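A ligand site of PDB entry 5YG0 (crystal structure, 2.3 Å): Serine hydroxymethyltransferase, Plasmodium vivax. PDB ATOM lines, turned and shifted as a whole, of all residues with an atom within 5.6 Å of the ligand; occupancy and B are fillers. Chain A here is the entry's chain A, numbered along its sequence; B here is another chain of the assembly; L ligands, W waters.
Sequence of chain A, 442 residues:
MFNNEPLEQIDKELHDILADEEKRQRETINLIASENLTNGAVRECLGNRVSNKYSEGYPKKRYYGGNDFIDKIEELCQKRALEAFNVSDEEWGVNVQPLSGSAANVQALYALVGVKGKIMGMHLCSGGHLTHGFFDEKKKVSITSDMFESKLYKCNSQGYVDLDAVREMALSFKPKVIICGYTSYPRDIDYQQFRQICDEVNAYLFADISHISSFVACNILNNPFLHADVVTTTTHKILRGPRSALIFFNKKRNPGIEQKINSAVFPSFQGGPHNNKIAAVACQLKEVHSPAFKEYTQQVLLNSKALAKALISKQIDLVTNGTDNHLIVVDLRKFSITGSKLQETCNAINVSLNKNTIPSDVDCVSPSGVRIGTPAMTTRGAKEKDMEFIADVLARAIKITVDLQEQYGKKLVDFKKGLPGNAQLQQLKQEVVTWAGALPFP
A fluorine (F1) of the ligand lies close to the backbone carbonyl oxygen (O) of Lys 355 (3.4 Å). The backbone carbonyl oxygen (O) of Cys 364 lies close to a fluorine (F2) of the ligand (2.9 Å). Merely in contact with the ligand: Arg 371 (3.3 Å), Leu 130 (3.4 Å), Pro 367 (3.4 Å), Val 141 (3.5 Å), Tyr 63 of chain B (3.6 Å), Ser 184 (3.6 Å), Asn 354 (3.7 Å), Tyr 64 of chain B (3.96 Å) and Pro 267 of chain B (3.99 Å). 18 residues have an atom within 4 Å of the ligand: Leu 124, Gly 128, His 129, Leu 130, Val 141, Thr 183, Ser 184, Asn 354, Lys 355, Asn 356, Thr 357, Cys 364, Pro 367, Arg 371, Glu 56 of chain B, Tyr 63 of chain B, Tyr 64 of chain B and Pro 267 of chain B.
Water W1 lies within hydrogen-bond range of the side-chain hydroxyl of Ser 184 (2.6 Å), the backbone carbonyl oxygen of Leu 124 (2.9 Å), a nitrogen (N3) of the ligand (2.9 Å), the backbone NH of Gly 127 (3.2 Å), the side-chain amide nitrogen of Asn 356 (3.3 Å) and the side-chain hydroxyl of Thr 357 (3.4 Å).
A nitrogen (N3) of the ligand is in hydrogen-bond range of the backbone carbonyl oxygen (O) of Leu 124, 3.3 Å away. An oxygen (O3) of the ligand is in hydrogen-bond range of the side-chain hydroxyl of Thr 183 (3.1 Å). A nitrogen (N2) of the ligand sits at hydrogen-bond distance from the side-chain hydroxyl (OG1) of Thr 357 (3.1 Å). A nitrogen (N4) of the ligand is in hydrogen-bond range of the side-chain carboxylate of Glu 56 of chain B, 2.9 Å away. N of Thr 357 sits at hydrogen-bond distance from N2 of the ligand. A ring nitrogen (NE2) of His 129 sits close to a nitrogen (N5) of the ligand. ND2 of Asn 356 is in hydrogen-bond range of N2 of the ligand, 3.2 Å away. O of Gly 128 is in hydrogen-bond range of N3 of the ligand, 3.0 Å away.
The side-chain carboxylate of Glu 56 of chain B is in hydrogen-bond range of the side-chain hydroxyl of Tyr 64 of chain B, 3.3 Å away. The backbone carbonyl oxygen (O) of Asn 354 sits at hydrogen-bond distance from the backbone NH (N) of Arg 371. The side-chain hydroxyl (OG1) of Thr 357 lies close to the backbone carbonyl oxygen (O) of Cys 125. The side-chain amide oxygen (OD1) of Asn 356 is in hydrogen-bond range of the side-chain hydroxyl (OG) of Ser 184 (3.3 Å). N of Ser 184 sits at hydrogen-bond distance from O of Gly 127 (3.1 Å). The backbone carbonyl oxygen of Thr 183 is in hydrogen-bond range of the guanidinium group of Arg 371 (3.4 Å). The backbone carbonyl oxygen (O) of Gly 127 sits at hydrogen-bond distance from the backbone NH (N) of Thr 183, 2.7 Å away. O of Glu 56 of chain B lies within hydrogen-bond range of N of Tyr 63 of chain B (3.2 Å).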
ATOM      1  N   LEU A 124      -0.413  20.477  23.577  1.00  0.00           N
ATOM      2  CA  LEU A 124      -0.100  21.793  24.161  1.00  0.00           C
ATOM      3  C   LEU A 124      -1.101  22.176  25.259  1.00  0.00           C
ATOM      4  O   LEU A 124      -0.715  22.307  26.430  1.00  0.00           O
ATOM      5  CB  LEU A 124      -0.033  22.860  23.054  1.00  0.00           C
ATOM      6  CG  LEU A 124       0.303  24.326  23.369  1.00  0.00           C
ATOM      7  CD1 LEU A 124       1.792  24.531  23.581  1.00  0.00           C
ATOM      8  CD2 LEU A 124      -0.168  25.227  22.243  1.00  0.00           C
ATOM      9  N   CYS A 125      -2.380  22.279  24.884  1.00  0.00           N
ATOM     10  CA  CYS A 125      -3.548  22.467  25.801  1.00  0.00           C
ATOM     11  C   CYS A 125      -3.597  21.630  27.078  1.00  0.00           C
ATOM     12  O   CYS A 125      -4.315  21.988  28.021  1.00  0.00           O
ATOM     13  CB  CYS A 125      -4.871  22.250  25.041  1.00  0.00           C
ATOM     14  SG  CYS A 125      -5.453  23.694  24.116  1.00  0.00           S
ATOM     15  N   GLY A 127      -0.619  20.600  28.681  1.00  0.00           N
ATOM     16  CA  GLY A 127       0.656  20.787  29.380  1.00  0.00           C
ATOM     17  C   GLY A 127       1.943  20.521  28.601  1.00  0.00           C
ATOM     18  O   GLY A 127       3.011  20.779  29.107  1.00  0.00           O
ATOM     19  N   GLY A 128       1.852  20.014  27.377  1.00  0.00           N
ATOM     20  CA  GLY A 128       3.045  19.671  26.598  1.00  0.00           C
ATOM     21  C   GLY A 128       3.665  20.863  25.887  1.00  0.00           C
ATOM     22  O   GLY A 128       3.013  21.883  25.739  1.00  0.00           O
ATOM     23  N   HIS A 129       4.923  20.731  25.466  1.00  0.00           N
ATOM     24  CA  HIS A 129       5.598  21.790  24.718  1.00  0.00           C
ATOM     25  C   HIS A 129       5.308  21.782  23.235  1.00  0.00           C
ATOM     26  O   HIS A 129       4.884  20.793  22.690  1.00  0.00           O
ATOM     27  CB  HIS A 129       7.121  21.748  24.955  1.00  0.00           C
ATOM     28  CG  HIS A 129       7.794  23.081  24.744  1.00  0.00           C
ATOM     29  ND1 HIS A 129       8.732  23.288  23.758  1.00  0.00           N
ATOM     30  CD2 HIS A 129       7.629  24.272  25.370  1.00  0.00           C
ATOM     31  CE1 HIS A 129       9.147  24.540  23.804  1.00  0.00           C
ATOM     32  NE2 HIS A 129       8.503  25.156  24.787  1.00  0.00           N
ATOM     33  N   LEU A 130       5.572  22.923  22.596  1.00  0.00           N
ATOM     34  CA  LEU A 130       5.552  23.044  21.140  1.00  0.00           C
ATOM     35  C   LEU A 130       6.443  22.009  20.455  1.00  0.00           C
ATOM     36  O   LEU A 130       6.075  21.478  19.416  1.00  0.00           O
ATOM     37  CB  LEU A 130       6.052  24.433  20.695  1.00  0.00           C
ATOM     38  CG  LEU A 130       5.357  25.692  21.231  1.00  0.00           C
ATOM     39  CD1 LEU A 130       6.334  26.870  21.263  1.00  0.00           C
ATOM     40  CD2 LEU A 130       4.127  26.029  20.418  1.00  0.00           C
ATOM     41  N   PHE A 134       3.593  19.613  18.527  1.00  0.00           N
ATOM     42  CA  PHE A 134       2.357  20.380  18.506  1.00  0.00           C
ATOM     43  C   PHE A 134       1.985  20.908  17.134  1.00  0.00           C
ATOM     44  O   PHE A 134       2.802  21.547  16.456  1.00  0.00           O
ATOM     45  CB  PHE A 134       2.382  21.590  19.430  1.00  0.00           C
ATOM     46  CG  PHE A 134       1.104  22.370  19.364  1.00  0.00           C
ATOM     47  CD1 PHE A 134      -0.106  21.768  19.721  1.00  0.00           C
ATOM     48  CD2 PHE A 134       1.085  23.667  18.858  1.00  0.00           C
ATOM     49  CE1 PHE A 134      -1.297  22.471  19.633  1.00  0.00           C
ATOM     50  CE2 PHE A 134      -0.117  24.357  18.755  1.00  0.00           C
ATOM     51  CZ  PHE A 134      -1.295  23.762  19.151  1.00  0.00           C
ATOM     52  N   VAL A 141       2.292  24.019  13.396  1.00  0.00           N
ATOM     53  CA  VAL A 141       2.779  25.105  14.214  1.00  0.00           C
ATOM     54  C   VAL A 141       4.246  24.894  14.647  1.00  0.00           C
ATOM     55  O   VAL A 141       5.067  25.819  14.577  1.00  0.00           O
ATOM     56  CB  VAL A 141       1.862  25.241  15.455  1.00  0.00           C
ATOM     57  CG1 VAL A 141       2.473  26.081  16.554  1.00  0.00           C
ATOM     58  CG2 VAL A 141       0.495  25.785  15.028  1.00  0.00           C
ATOM     59  N   THR A 183       5.571  21.256  29.953  1.00  0.00           N
ATOM     60  CA  THR A 183       5.741  22.712  30.184  1.00  0.00           C
ATOM     61  C   THR A 183       4.851  23.268  31.319  1.00  0.00           C
ATOM     62  O   THR A 183       5.359  23.973  32.198  1.00  0.00           O
ATOM     63  CB  THR A 183       5.687  23.602  28.906  1.00  0.00           C
ATOM     64  OG1 THR A 183       4.728  24.645  29.053  1.00  0.00           O
ATOM     65  CG2 THR A 183       5.357  22.851  27.700  1.00  0.00           C
ATOM     66  N   SER A 184       3.573  22.911  31.350  1.00  0.00           N
ATOM     67  CA  SER A 184       2.663  23.361  32.427  1.00  0.00           C
ATOM     68  C   SER A 184       1.754  22.235  32.896  1.00  0.00           C
ATOM     69  O   SER A 184       0.529  22.313  32.823  1.00  0.00           O
ATOM     70  CB  SER A 184       1.862  24.582  31.962  1.00  0.00           C
ATOM     71  OG  SER A 184       1.303  24.328  30.708  1.00  0.00           O
ATOM     72  N   ASN A 354       2.104  34.095  33.317  1.00  0.00           N
ATOM     73  CA  ASN A 354       1.664  33.910  31.951  1.00  0.00           C
ATOM     74  C   ASN A 354       0.294  33.261  31.871  1.00  0.00           C
ATOM     75  O   ASN A 354      -0.094  32.479  32.739  1.00  0.00           O
ATOM     76  CB  ASN A 354       2.689  33.110  31.126  1.00  0.00           C
ATOM     77  CG  ASN A 354       2.771  31.660  31.538  1.00  0.00           C
ATOM     78  OD1 ASN A 354       3.500  31.298  32.461  1.00  0.00           O
ATOM     79  ND2 ASN A 354       2.009  30.812  30.846  1.00  0.00           N
ATOM     80  N   LYS A 355      -0.418  33.624  30.814  1.00  0.00           N
ATOM     81  CA  LYS A 355      -1.645  32.944  30.448  1.00  0.00           C
ATOM     82  C   LYS A 355      -1.365  31.495  30.151  1.00  0.00           C
ATOM     83  O   LYS A 355      -0.234  31.118  29.786  1.00  0.00           O
ATOM     84  CB  LYS A 355      -2.391  33.593  29.266  1.00  0.00           C
ATOM     85  CG  LYS A 355      -1.549  34.392  28.262  1.00  0.00           C
ATOM     86  CD  LYS A 355      -2.197  34.485  26.893  1.00  0.00           C
ATOM     87  CE  LYS A 355      -1.759  35.746  26.140  1.00  0.00           C
ATOM     88  NZ  LYS A 355      -2.035  35.568  24.687  1.00  0.00           N
ATOM     89  N   ASN A 356      -2.385  30.669  30.333  1.00  0.00           N
ATOM     90  CA  ASN A 356      -2.239  29.229  30.161  1.00  0.00           C
ATOM     91  C   ASN A 356      -3.577  28.572  29.870  1.00  0.00           C
ATOM     92  O   ASN A 356      -4.599  28.931  30.450  1.00  0.00           O
ATOM     93  CB  ASN A 356      -1.612  28.612  31.411  1.00  0.00           C
ATOM     94  CG  ASN A 356      -0.747  27.407  31.079  1.00  0.00           C
ATOM     95  OD1 ASN A 356       0.488  27.491  31.025  1.00  0.00           O
ATOM     96  ND2 ASN A 356      -1.398  26.301  30.759  1.00  0.00           N
ATOM     97  N   THR A 357      -3.572  27.581  28.990  1.00  0.00           N
ATOM     98  CA  THR A 357      -4.739  26.751  28.742  1.00  0.00           C
ATOM     99  C   THR A 357      -5.108  25.846  29.946  1.00  0.00           C
ATOM    100  O   THR A 357      -4.299  25.672  30.888  1.00  0.00           O
ATOM    101  CB  THR A 357      -4.479  25.840  27.540  1.00  0.00           C
ATOM    102  OG1 THR A 357      -3.253  25.135  27.744  1.00  0.00           O
ATOM    103  CG2 THR A 357      -4.399  26.662  26.265  1.00  0.00           C
ATOM    104  N   ASP A 363      -9.848  26.364  22.552  1.00  0.00           N
ATOM    105  CA  ASP A 363      -8.906  27.247  21.832  1.00  0.00           C
ATOM    106  C   ASP A 363      -7.783  27.807  22.716  1.00  0.00           C
ATOM    107  O   ASP A 363      -7.926  27.927  23.938  1.00  0.00           O
ATOM    108  CB  ASP A 363      -9.629  28.438  21.174  1.00  0.00           C
ATOM    109  CG  ASP A 363     -10.957  28.071  20.550  1.00  0.00           C
ATOM    110  OD1 ASP A 363     -11.878  27.669  21.290  1.00  0.00           O
ATOM    111  OD2 ASP A 363     -11.089  28.206  19.305  1.00  0.00           O
ATOM    112  N   CYS A 364      -6.689  28.170  22.060  1.00  0.00           N
ATOM    113  CA  CYS A 364      -5.538  28.841  22.691  1.00  0.00           C
ATOM    114  C   CYS A 364      -5.677  30.370  22.657  1.00  0.00           C
ATOM    115  O   CYS A 364      -4.961  31.058  23.389  1.00  0.00           O
ATOM    116  CB  CYS A 364      -4.251  28.415  22.004  1.00  0.00           C
ATOM    117  SG  CYS A 364      -4.090  26.603  21.935  1.00  0.00           S
ATOM    118  N   VAL A 365      -6.534  30.903  21.787  1.00  0.00           N
ATOM    119  CA  VAL A 365      -7.109  32.247  21.955  1.00  0.00           C
ATOM    120  C   VAL A 365      -8.213  32.134  23.013  1.00  0.00           C
ATOM    121  O   VAL A 365      -9.087  31.258  22.923  1.00  0.00           O
ATOM    122  CB  VAL A 365      -7.671  32.814  20.633  1.00  0.00           C
ATOM    123  CG1 VAL A 365      -8.478  34.098  20.862  1.00  0.00           C
ATOM    124  CG2 VAL A 365      -6.552  33.063  19.632  1.00  0.00           C
ATOM    125  N   PRO A 367      -7.393  31.584  26.519  1.00  0.00           N
ATOM    126  CA  PRO A 367      -7.051  30.535  27.501  1.00  0.00           C
ATOM    127  C   PRO A 367      -7.663  30.840  28.878  1.00  0.00           C
ATOM    128  O   PRO A 367      -7.658  32.007  29.312  1.00  0.00           O
ATOM    129  CB  PRO A 367      -5.526  30.592  27.575  1.00  0.00           C
ATOM    130  CG  PRO A 367      -5.197  32.004  27.245  1.00  0.00           C
ATOM    131  CD  PRO A 367      -6.221  32.445  26.228  1.00  0.00           C
ATOM    132  N   ARG A 371      -0.604  30.344  34.691  1.00  0.00           N
ATOM    133  CA  ARG A 371       0.336  29.507  35.356  1.00  0.00           C
ATOM    134  C   ARG A 371       1.227  30.371  36.214  1.00  0.00           C
ATOM    135  O   ARG A 371       1.612  31.466  35.797  1.00  0.00           O
ATOM    136  CB  ARG A 371       1.154  28.747  34.317  1.00  0.00           C
ATOM    137  CG  ARG A 371       2.157  27.746  34.839  1.00  0.00           C
ATOM    138  CD  ARG A 371       3.086  27.288  33.721  1.00  0.00           C
ATOM    139  NE  ARG A 371       4.106  28.285  33.418  1.00  0.00           N
ATOM    140  CZ  ARG A 371       4.948  28.240  32.383  1.00  0.00           C
ATOM    141  NH1 ARG A 371       4.918  27.233  31.521  1.00  0.00           N
ATOM    142  NH2 ARG A 371       5.825  29.214  32.218  1.00  0.00           N
ATOM    143  N   GLU B  56       8.878  35.072  24.759  1.00  0.00           N
ATOM    144  CA  GLU B  56       8.416  34.318  23.586  1.00  0.00           C
ATOM    145  C   GLU B  56       7.352  35.060  22.777  1.00  0.00           C
ATOM    146  O   GLU B  56       6.415  35.637  23.341  1.00  0.00           O
ATOM    147  CB  GLU B  56       7.827  33.036  24.102  1.00  0.00           C
ATOM    148  CG  GLU B  56       7.919  31.837  23.222  1.00  0.00           C
ATOM    149  CD  GLU B  56       8.094  30.553  24.016  1.00  0.00           C
ATOM    150  OE1 GLU B  56       7.578  29.509  23.571  1.00  0.00           O
ATOM    151  OE2 GLU B  56       8.744  30.576  25.072  1.00  0.00           O
ATOM    152  N   TYR B  63       3.924  36.129  25.232  1.00  0.00           N
ATOM    153  CA  TYR B  63       3.197  35.143  26.012  1.00  0.00           C
ATOM    154  C   TYR B  63       3.553  35.233  27.478  1.00  0.00           C
ATOM    155  O   TYR B  63       3.098  34.417  28.264  1.00  0.00           O
ATOM    156  CB  TYR B  63       3.457  33.746  25.472  1.00  0.00           C
ATOM    157  CG  TYR B  63       2.782  33.531  24.138  1.00  0.00           C
ATOM    158  CD1 TYR B  63       3.369  33.967  22.975  1.00  0.00           C
ATOM    159  CD2 TYR B  63       1.542  32.925  24.061  1.00  0.00           C
ATOM    160  CE1 TYR B  63       2.750  33.795  21.758  1.00  0.00           C
ATOM    161  CE2 TYR B  63       0.909  32.750  22.843  1.00  0.00           C
ATOM    162  CZ  TYR B  63       1.507  33.189  21.709  1.00  0.00           C
ATOM    163  OH  TYR B  63       0.881  33.005  20.513  1.00  0.00           O
ATOM    164  N   TYR B  64       4.384  36.199  27.841  1.00  0.00           N
ATOM    165  CA  TYR B  64       4.694  36.463  29.225  1.00  0.00           C
ATOM    166  C   TYR B  64       4.490  37.945  29.492  1.00  0.00           C
ATOM    167  O   TYR B  64       4.476  38.788  28.557  1.00  0.00           O
ATOM    168  CB  TYR B  64       6.129  36.021  29.565  1.00  0.00           C
ATOM    169  CG  TYR B  64       6.378  34.584  29.159  1.00  0.00           C
ATOM    170  CD1 TYR B  64       6.744  34.289  27.870  1.00  0.00           C
ATOM    171  CD2 TYR B  64       6.208  33.536  30.060  1.00  0.00           C
ATOM    172  CE1 TYR B  64       6.934  32.984  27.466  1.00  0.00           C
ATOM    173  CE2 TYR B  64       6.385  32.219  29.669  1.00  0.00           C
ATOM    174  CZ  TYR B  64       6.762  31.946  28.367  1.00  0.00           C
ATOM    175  OH  TYR B  64       6.994  30.677  27.895  1.00  0.00           O
ATOM    176  N   PHE B 266       9.785  31.698  15.238  1.00  0.00           N
ATOM    177  CA  PHE B 266       8.926  31.253  16.317  1.00  0.00           C
ATOM    178  C   PHE B 266       7.491  31.215  15.860  1.00  0.00           C
ATOM    179  O   PHE B 266       7.046  32.182  15.281  1.00  0.00           O
ATOM    180  CB  PHE B 266       9.014  32.195  17.510  1.00  0.00           C
ATOM    181  CG  PHE B 266       8.020  31.868  18.577  1.00  0.00           C
ATOM    182  CD1 PHE B 266       8.286  30.835  19.476  1.00  0.00           C
ATOM    183  CD2 PHE B 266       6.782  32.525  18.642  1.00  0.00           C
ATOM    184  CE1 PHE B 266       7.347  30.485  20.434  1.00  0.00           C
ATOM    185  CE2 PHE B 266       5.851  32.166  19.608  1.00  0.00           C
ATOM    186  CZ  PHE B 266       6.151  31.150  20.502  1.00  0.00           C
ATOM    187  N   PRO B 267       6.711  30.170  16.153  1.00  0.00           N
ATOM    188  CA  PRO B 267       7.081  29.022  16.997  1.00  0.00           C
ATOM    189  C   PRO B 267       7.525  27.776  16.236  1.00  0.00           C
ATOM    190  O   PRO B 267       7.585  26.701  16.828  1.00  0.00           O
ATOM    191  CB  PRO B 267       5.767  28.734  17.720  1.00  0.00           C
ATOM    192  CG  PRO B 267       4.722  29.058  16.688  1.00  0.00           C
ATOM    193  CD  PRO B 267       5.295  30.085  15.740  1.00  0.00           C
HETATM  194  C1  LIG L   1       0.676  29.366  19.001  1.00  0.00           C
HETATM  195  C2  LIG L   1       0.815  29.057  17.495  1.00  0.00           C
HETATM  196  C3  LIG L   1       1.853  29.391  21.183  1.00  0.00           C
HETATM  197  C4  LIG L   1       0.556  30.201  16.533  1.00  0.00           C
HETATM  198  C5  LIG L   1      -0.749  28.889  20.958  1.00  0.00           C
HETATM  199  C6  LIG L   1      -0.451  28.508  19.529  1.00  0.00           C
HETATM  200  C7  LIG L   1       1.953  29.005  19.710  1.00  0.00           C
HETATM  201  N1  LIG L   1       0.508  29.033  21.720  1.00  0.00           N
HETATM  202  F1  LIG L   1      -2.092  30.494  26.959  1.00  0.00           F
HETATM  203  C8  LIG L   1      -2.104  30.395  25.640  1.00  0.00           C
HETATM  204  F2  LIG L   1      -3.153  29.726  25.265  1.00  0.00           F
HETATM  205  F3  LIG L   1      -2.236  31.580  25.077  1.00  0.00           F
HETATM  206  C9  LIG L   1      -0.876  29.717  25.085  1.00  0.00           C
HETATM  207  C10 LIG L   1       0.113  29.186  25.909  1.00  0.00           C
HETATM  208  C11 LIG L   1      -0.717  29.648  23.708  1.00  0.00           C
HETATM  209  C12 LIG L   1       0.393  29.039  23.122  1.00  0.00           C
HETATM  210  O1  LIG L   1       0.144  29.884  15.390  1.00  0.00           O
HETATM  211  O2  LIG L   1       0.786  31.386  16.891  1.00  0.00           O
HETATM  212  C13 LIG L   1       1.369  28.496  23.973  1.00  0.00           C
HETATM  213  C14 LIG L   1       1.272  28.567  25.377  1.00  0.00           C
HETATM  214  C15 LIG L   1       2.319  27.946  26.311  1.00  0.00           C
HETATM  215  C16 LIG L   1       2.632  28.757  27.600  1.00  0.00           C
HETATM  216  C17 LIG L   1       3.588  28.051  28.614  1.00  0.00           C
HETATM  217  C18 LIG L   1       3.098  30.216  27.358  1.00  0.00           C
HETATM  218  C19 LIG L   1       1.698  26.627  26.768  1.00  0.00           C
HETATM  219  C20 LIG L   1       0.522  26.642  27.231  1.00  0.00           C
HETATM  220  N2  LIG L   1      -0.554  26.644  27.652  1.00  0.00           N
HETATM  221  C21 LIG L   1       2.371  25.455  26.712  1.00  0.00           C
HETATM  222  N3  LIG L   1       1.845  24.304  27.125  1.00  0.00           N
HETATM  223  C22 LIG L   1       3.605  27.702  25.596  1.00  0.00           C
HETATM  224  C23 LIG L   1       4.535  28.530  24.776  1.00  0.00           C
HETATM  225  C24 LIG L   1       4.422  29.985  24.390  1.00  0.00           C
HETATM  226  N4  LIG L   1       5.537  27.704  24.410  1.00  0.00           N
HETATM  227  N5  LIG L   1       5.407  26.380  24.862  1.00  0.00           N
HETATM  228  C25 LIG L   1       4.276  26.408  25.562  1.00  0.00           C
HETATM  229  O3  LIG L   1       3.728  25.359  26.228  1.00  0.00           O
HETATM  230  O   HOH W   1      -0.391  23.741  28.872  1.00  0.00           O
